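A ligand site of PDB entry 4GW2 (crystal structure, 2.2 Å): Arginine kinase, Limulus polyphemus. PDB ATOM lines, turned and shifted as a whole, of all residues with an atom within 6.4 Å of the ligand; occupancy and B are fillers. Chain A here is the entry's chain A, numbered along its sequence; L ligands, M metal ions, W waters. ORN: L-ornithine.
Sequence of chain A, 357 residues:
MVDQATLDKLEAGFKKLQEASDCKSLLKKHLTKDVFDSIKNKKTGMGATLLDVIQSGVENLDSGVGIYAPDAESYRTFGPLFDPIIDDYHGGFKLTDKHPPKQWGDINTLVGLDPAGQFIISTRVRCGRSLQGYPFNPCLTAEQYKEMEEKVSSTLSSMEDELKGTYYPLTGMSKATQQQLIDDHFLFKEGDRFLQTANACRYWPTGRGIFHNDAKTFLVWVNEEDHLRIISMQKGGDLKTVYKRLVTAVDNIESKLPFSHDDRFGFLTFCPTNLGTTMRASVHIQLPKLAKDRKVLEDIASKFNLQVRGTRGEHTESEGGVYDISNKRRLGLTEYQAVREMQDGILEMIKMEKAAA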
ATOM      1  N   SER A  25      36.827 -21.064 -22.267  1.00  0.00           N
ATOM      2  CA  SER A  25      36.335 -22.391 -21.910  1.00  0.00           C
ATOM      3  C   SER A  25      37.234 -23.134 -20.894  1.00  0.00           C
ATOM      4  O   SER A  25      38.427 -22.872 -20.807  1.00  0.00           O
ATOM      5  CB  SER A  25      36.112 -23.205 -23.185  1.00  0.00           C
ATOM      6  OG  SER A  25      37.305 -23.386 -23.919  1.00  0.00           O
ATOM      7  N   SER A  56      34.911 -31.085 -29.717  1.00  0.00           N
ATOM      8  CA  SER A  56      33.823 -30.118 -29.712  1.00  0.00           C
ATOM      9  C   SER A  56      34.323 -28.779 -29.179  1.00  0.00           C
ATOM     10  O   SER A  56      33.909 -27.721 -29.661  1.00  0.00           O
ATOM     11  CB  SER A  56      32.670 -30.599 -28.822  1.00  0.00           C
ATOM     12  OG  SER A  56      31.642 -29.636 -28.763  1.00  0.00           O
ATOM     13  N   ASP A  62      33.977 -20.907 -28.327  1.00  0.00           N
ATOM     14  CA  ASP A  62      33.022 -20.231 -27.444  1.00  0.00           C
ATOM     15  C   ASP A  62      32.387 -21.196 -26.435  1.00  0.00           C
ATOM     16  O   ASP A  62      31.533 -20.802 -25.651  1.00  0.00           O
ATOM     17  CB  ASP A  62      31.963 -19.507 -28.267  1.00  0.00           C
ATOM     18  CG  ASP A  62      31.189 -20.424 -29.193  1.00  0.00           C
ATOM     19  OD1 ASP A  62      31.728 -21.500 -29.548  1.00  0.00           O
ATOM     20  OD2 ASP A  62      30.054 -20.080 -29.566  1.00  0.00           O
ATOM     21  N   SER A  63      32.795 -22.463 -26.484  1.00  0.00           N
ATOM     22  CA  SER A  63      32.333 -23.454 -25.515  1.00  0.00           C
ATOM     23  C   SER A  63      32.593 -22.935 -24.109  1.00  0.00           C
ATOM     24  O   SER A  63      33.561 -22.220 -23.873  1.00  0.00           O
ATOM     25  CB  SER A  63      33.060 -24.797 -25.714  1.00  0.00           C
ATOM     26  OG  SER A  63      32.716 -25.395 -26.952  1.00  0.00           O
ATOM     27  N   GLY A  64      31.704 -23.260 -23.170  1.00  0.00           N
ATOM     28  CA  GLY A  64      31.983 -23.001 -21.768  1.00  0.00           C
ATOM     29  C   GLY A  64      32.819 -24.099 -21.162  1.00  0.00           C
ATOM     30  O   GLY A  64      33.630 -23.855 -20.268  1.00  0.00           O
ATOM     31  N   VAL A  65      32.631 -25.321 -21.652  1.00  0.00           N
ATOM     32  CA  VAL A  65      33.311 -26.494 -21.114  1.00  0.00           C
ATOM     33  C   VAL A  65      34.209 -27.160 -22.146  1.00  0.00           C
ATOM     34  O   VAL A  65      35.432 -27.219 -21.984  1.00  0.00           O
ATOM     35  CB  VAL A  65      32.324 -27.522 -20.551  1.00  0.00           C
ATOM     36  CG1 VAL A  65      33.061 -28.722 -19.980  1.00  0.00           C
ATOM     37  CG2 VAL A  65      31.442 -26.873 -19.479  1.00  0.00           C
ATOM     38  N   GLY A  66      33.609 -27.686 -23.205  1.00  0.00           N
ATOM     39  CA  GLY A  66      34.352 -28.133 -24.372  1.00  0.00           C
ATOM     40  C   GLY A  66      34.639 -29.619 -24.491  1.00  0.00           C
ATOM     41  O   GLY A  66      35.284 -30.031 -25.449  1.00  0.00           O
ATOM     42  N   ILE A  67      34.183 -30.410 -23.536  1.00  0.00           N
ATOM     43  CA  ILE A  67      34.441 -31.852 -23.588  1.00  0.00           C
ATOM     44  C   ILE A  67      33.204 -32.706 -23.316  1.00  0.00           C
ATOM     45  O   ILE A  67      32.244 -32.256 -22.687  1.00  0.00           O
ATOM     46  CB  ILE A  67      35.556 -32.270 -22.596  1.00  0.00           C
ATOM     47  CG1 ILE A  67      35.111 -32.028 -21.155  1.00  0.00           C
ATOM     48  CG2 ILE A  67      36.854 -31.525 -22.906  1.00  0.00           C
ATOM     49  CD1 ILE A  67      36.076 -32.576 -20.140  1.00  0.00           C
ATOM     50  N   TYR A  68      33.236 -33.940 -23.796  1.00  0.00           N
ATOM     51  CA  TYR A  68      32.173 -34.907 -23.540  1.00  0.00           C
ATOM     52  C   TYR A  68      32.833 -36.268 -23.333  1.00  0.00           C
ATOM     53  O   TYR A  68      33.970 -36.480 -23.750  1.00  0.00           O
ATOM     54  CB  TYR A  68      31.237 -35.001 -24.740  1.00  0.00           C
ATOM     55  CG  TYR A  68      30.400 -33.771 -25.008  1.00  0.00           C
ATOM     56  CD1 TYR A  68      30.841 -32.799 -25.890  1.00  0.00           C
ATOM     57  CD2 TYR A  68      29.170 -33.603 -24.396  1.00  0.00           C
ATOM     58  CE1 TYR A  68      30.077 -31.666 -26.140  1.00  0.00           C
ATOM     59  CE2 TYR A  68      28.393 -32.488 -24.648  1.00  0.00           C
ATOM     60  CZ  TYR A  68      28.848 -31.527 -25.520  1.00  0.00           C
ATOM     61  OH  TYR A  68      28.075 -30.426 -25.773  1.00  0.00           O
ATOM     62  N   ARG A 126      14.513 -30.845 -14.836  1.00  0.00           N
ATOM     63  CA  ARG A 126      14.867 -32.039 -15.603  1.00  0.00           C
ATOM     64  C   ARG A 126      15.950 -32.877 -14.953  1.00  0.00           C
ATOM     65  O   ARG A 126      16.761 -32.378 -14.164  1.00  0.00           O
ATOM     66  CB  ARG A 126      15.209 -31.686 -17.066  1.00  0.00           C
ATOM     67  CG  ARG A 126      16.438 -30.826 -17.302  1.00  0.00           C
ATOM     68  CD  ARG A 126      17.746 -31.628 -17.268  1.00  0.00           C
ATOM     69  NE  ARG A 126      18.860 -30.873 -17.835  1.00  0.00           N
ATOM     70  CZ  ARG A 126      20.147 -31.097 -17.596  1.00  0.00           C
ATOM     71  NH1 ARG A 126      21.064 -30.354 -18.211  1.00  0.00           N
ATOM     72  NH2 ARG A 126      20.531 -32.015 -16.731  1.00  0.00           N
ATOM     73  N   PHE A 194      27.641 -27.705 -30.980  1.00  0.00           N
ATOM     74  CA  PHE A 194      28.503 -28.266 -29.940  1.00  0.00           C
ATOM     75  C   PHE A 194      28.360 -29.781 -29.871  1.00  0.00           C
ATOM     76  O   PHE A 194      29.347 -30.509 -29.745  1.00  0.00           O
ATOM     77  CB  PHE A 194      28.141 -27.672 -28.572  1.00  0.00           C
ATOM     78  CG  PHE A 194      28.248 -26.166 -28.523  1.00  0.00           C
ATOM     79  CD1 PHE A 194      27.138 -25.371 -28.749  1.00  0.00           C
ATOM     80  CD2 PHE A 194      29.462 -25.550 -28.246  1.00  0.00           C
ATOM     81  CE1 PHE A 194      27.236 -23.999 -28.713  1.00  0.00           C
ATOM     82  CE2 PHE A 194      29.561 -24.178 -28.210  1.00  0.00           C
ATOM     83  CZ  PHE A 194      28.447 -23.392 -28.441  1.00  0.00           C
ATOM     84  N   LEU A 195      27.121 -30.261 -29.970  1.00  0.00           N
ATOM     85  CA  LEU A 195      26.841 -31.697 -29.971  1.00  0.00           C
ATOM     86  C   LEU A 195      27.283 -32.327 -31.285  1.00  0.00           C
ATOM     87  O   LEU A 195      27.842 -33.427 -31.319  1.00  0.00           O
ATOM     88  CB  LEU A 195      25.346 -31.934 -29.749  1.00  0.00           C
ATOM     89  CG  LEU A 195      24.805 -31.704 -28.332  1.00  0.00           C
ATOM     90  CD1 LEU A 195      23.282 -31.733 -28.325  1.00  0.00           C
ATOM     91  CD2 LEU A 195      25.367 -32.718 -27.351  1.00  0.00           C
ATOM     92  N   GLU A 225      20.905 -35.425 -26.260  1.00  0.00           N
ATOM     93  CA  GLU A 225      22.235 -35.387 -25.664  1.00  0.00           C
ATOM     94  C   GLU A 225      22.456 -36.607 -24.762  1.00  0.00           C
ATOM     95  O   GLU A 225      23.534 -37.202 -24.756  1.00  0.00           O
ATOM     96  CB  GLU A 225      22.445 -34.094 -24.872  1.00  0.00           C
ATOM     97  CG  GLU A 225      23.762 -34.042 -24.105  1.00  0.00           C
ATOM     98  CD  GLU A 225      24.009 -32.697 -23.447  1.00  0.00           C
ATOM     99  OE1 GLU A 225      24.730 -32.666 -22.423  1.00  0.00           O
ATOM    100  OE2 GLU A 225      23.517 -31.669 -23.954  1.00  0.00           O
ATOM    101  N   ARG A 229      16.101 -37.700 -21.181  1.00  0.00           N
ATOM    102  CA  ARG A 229      15.930 -36.556 -20.296  1.00  0.00           C
ATOM    103  C   ARG A 229      14.491 -36.589 -19.833  1.00  0.00           C
ATOM    104  O   ARG A 229      13.573 -36.670 -20.649  1.00  0.00           O
ATOM    105  CB  ARG A 229      16.216 -35.235 -21.016  1.00  0.00           C
ATOM    106  CG  ARG A 229      17.679 -35.026 -21.442  1.00  0.00           C
ATOM    107  CD  ARG A 229      18.584 -34.808 -20.227  1.00  0.00           C
ATOM    108  NE  ARG A 229      19.953 -34.433 -20.590  1.00  0.00           N
ATOM    109  CZ  ARG A 229      20.325 -33.244 -21.052  1.00  0.00           C
ATOM    110  NH1 ARG A 229      19.434 -32.270 -21.181  1.00  0.00           N
ATOM    111  NH2 ARG A 229      21.595 -33.021 -21.363  1.00  0.00           N
ATOM    112  N   CYS A 271      27.663 -35.356 -20.868  1.00  0.00           N
ATOM    113  CA  CYS A 271      28.456 -34.188 -20.492  1.00  0.00           C
ATOM    114  C   CYS A 271      28.804 -34.245 -19.004  1.00  0.00           C
ATOM    115  O   CYS A 271      27.970 -34.630 -18.181  1.00  0.00           O
ATOM    116  CB  CYS A 271      27.720 -32.880 -20.811  1.00  0.00           C
ATOM    117  SG  CYS A 271      28.599 -31.348 -20.363  1.00  0.00           S
ATOM    118  N   THR A 273      29.067 -31.863 -16.973  1.00  0.00           N
ATOM    119  CA  THR A 273      28.275 -30.916 -16.220  1.00  0.00           C
ATOM    120  C   THR A 273      26.988 -31.536 -15.673  1.00  0.00           C
ATOM    121  O   THR A 273      26.356 -30.990 -14.767  1.00  0.00           O
ATOM    122  CB  THR A 273      27.845 -29.724 -17.089  1.00  0.00           C
ATOM    123  OG1 THR A 273      27.006 -30.200 -18.151  1.00  0.00           O
ATOM    124  CG2 THR A 273      29.057 -29.009 -17.671  1.00  0.00           C
ATOM    125  N   ASN A 274      26.612 -32.694 -16.199  1.00  0.00           N
ATOM    126  CA  ASN A 274      25.315 -33.300 -15.880  1.00  0.00           C
ATOM    127  C   ASN A 274      25.411 -34.503 -14.952  1.00  0.00           C
ATOM    128  O   ASN A 274      24.430 -35.220 -14.739  1.00  0.00           O
ATOM    129  CB  ASN A 274      24.559 -33.639 -17.165  1.00  0.00           C
ATOM    130  CG  ASN A 274      23.987 -32.417 -17.854  1.00  0.00           C
ATOM    131  OD1 ASN A 274      23.439 -31.521 -17.203  1.00  0.00           O
ATOM    132  ND2 ASN A 274      24.132 -32.358 -19.169  1.00  0.00           N
ATOM    133  N   ARG A 309      20.943 -18.499 -18.913  1.00  0.00           N
ATOM    134  CA  ARG A 309      20.856 -18.903 -20.309  1.00  0.00           C
ATOM    135  C   ARG A 309      19.794 -18.061 -21.023  1.00  0.00           C
ATOM    136  O   ARG A 309      18.953 -17.453 -20.384  1.00  0.00           O
ATOM    137  CB  ARG A 309      20.485 -20.374 -20.404  1.00  0.00           C
ATOM    138  CG  ARG A 309      21.530 -21.305 -19.840  1.00  0.00           C
ATOM    139  CD  ARG A 309      21.042 -22.741 -19.840  1.00  0.00           C
ATOM    140  NE  ARG A 309      22.045 -23.632 -19.278  1.00  0.00           N
ATOM    141  CZ  ARG A 309      22.183 -24.922 -19.602  1.00  0.00           C
ATOM    142  NH1 ARG A 309      21.346 -25.480 -20.458  1.00  0.00           N
ATOM    143  NH2 ARG A 309      23.137 -25.643 -19.030  1.00  0.00           N
ATOM    144  N   GLU A 314      20.712 -22.695 -23.674  1.00  0.00           N
ATOM    145  CA  GLU A 314      22.112 -22.275 -23.633  1.00  0.00           C
ATOM    146  C   GLU A 314      22.572 -21.755 -24.999  1.00  0.00           C
ATOM    147  O   GLU A 314      22.089 -22.218 -26.029  1.00  0.00           O
ATOM    148  CB  GLU A 314      22.989 -23.423 -23.155  1.00  0.00           C
ATOM    149  CG  GLU A 314      22.833 -24.701 -23.963  1.00  0.00           C
ATOM    150  CD  GLU A 314      23.889 -25.736 -23.623  1.00  0.00           C
ATOM    151  OE1 GLU A 314      24.675 -25.491 -22.695  1.00  0.00           O
ATOM    152  OE2 GLU A 314      23.902 -26.810 -24.263  1.00  0.00           O
ATOM    153  N   HIS A 315      23.517 -20.801 -24.992  1.00  0.00           N
ATOM    154  CA  HIS A 315      24.088 -20.269 -26.237  1.00  0.00           C
ATOM    155  C   HIS A 315      23.076 -19.541 -27.098  1.00  0.00           C
ATOM    156  O   HIS A 315      23.222 -19.451 -28.321  1.00  0.00           O
ATOM    157  CB  HIS A 315      24.819 -21.352 -27.053  1.00  0.00           C
ATOM    158  CG  HIS A 315      25.855 -22.082 -26.267  1.00  0.00           C
ATOM    159  ND1 HIS A 315      25.863 -23.450 -26.105  1.00  0.00           N
ATOM    160  CD2 HIS A 315      26.964 -21.628 -25.626  1.00  0.00           C
ATOM    161  CE1 HIS A 315      26.904 -23.799 -25.374  1.00  0.00           C
ATOM    162  NE2 HIS A 315      27.594 -22.712 -25.086  1.00  0.00           N
HETATM  163  N   ORN L   1      29.621 -28.378 -24.582  1.00  0.00           N
HETATM  164  CA  ORN L   1      28.903 -27.102 -24.585  1.00  0.00           C
HETATM  165  CB  ORN L   1      27.594 -27.261 -23.779  1.00  0.00           C
HETATM  166  CG  ORN L   1      27.828 -27.740 -22.348  1.00  0.00           C
HETATM  167  CD  ORN L   1      26.491 -27.650 -21.577  1.00  0.00           C
HETATM  168  NE  ORN L   1      25.835 -28.970 -21.526  1.00  0.00           N
HETATM  169  C   ORN L   1      29.792 -26.011 -23.886  1.00  0.00           C
HETATM  170  O   ORN L   1      30.862 -26.392 -23.387  1.00  0.00           O
HETATM  171  OXT ORN L   1      29.358 -24.840 -23.884  1.00  0.00           O
HETATM  172 MG    MG M   1      20.059 -29.301 -23.987  1.00  0.00          MG
HETATM  173  O   HOH W   1      28.251 -23.627 -21.561  1.00  0.00           O
HETATM  174  O   HOH W   2      30.492 -29.996 -22.520  1.00  0.00           O
HETATM  175  O   HOH W   3      31.539 -27.850 -26.441  1.00  0.00           O
HETATM  176  O   HOH W   4      25.555 -30.001 -24.808  1.00  0.00           O
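N of Val 65 is in hydrogen-bond range of O of the ligand (2.7 Å). N of the ligand sits at hydrogen-bond distance from OH of Tyr 68, 2.8 Å away. The backbone NH (N) of Gly 64 lies within hydrogen-bond range of an oxygen (OXT) of the ligand (2.9 Å). NE2 of His 315 sits at hydrogen-bond distance from OXT of the ligand (3.0 Å). NE of the ligand is in salt-bridge range of OE1 of Glu 314, at 3.8 Å. N of Gly 66 sits at hydrogen-bond distance from O of the ligand, 3.0 Å away. NE of the ligand is in salt-bridge range of OE1 of Glu 225, 3.96 Å away.
The side-chain carboxylate (OE1) of Glu 314 lies within salt-bridge range of the guanidinium group (NH2) of Arg 309, 3.98 Å away. SG of Cys 271 sits at hydrogen-bond distance from OG1 of Thr 273. The side-chain amide nitrogen (ND2) of Asn 274 is in hydrogen-bond range of the side-chain carboxylate (OE1) of Glu 225, at 3.3 Å. The guanidinium group (NH2) of Arg 229 lies within salt-bridge range of the side-chain carboxylate (OE1) of Glu 225.
Residues that only touch the ligand: Ser 63, Thr 273 and Cys 271. Hydrophobic or aromatic side chains within 4 Å of the ligand: Val 65, Tyr 68 and His 315. Within 4 Å of the ligand: Ser 63, Gly 64, Val 65, Gly 66, Tyr 68, Glu 225, Cys 271, Thr 273, Glu 314 and His 315.
Water W3 lies within hydrogen-bond range of N of the ligand, OG of Ser 63 and OG of Ser 56. Water W2 lies within hydrogen-bond range of a nitrogen (N) of the ligand (2.8 Å), the backbone carbonyl oxygen of Ile 67 (2.9 Å) and the side-chain sulfur of Cys 271 (3.2 Å). Water W4 lies within hydrogen-bond range of OH of Tyr 68 (2.7 Å), OE2 of Glu 225 (2.8 Å) and NE of the ligand (3.5 Å).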
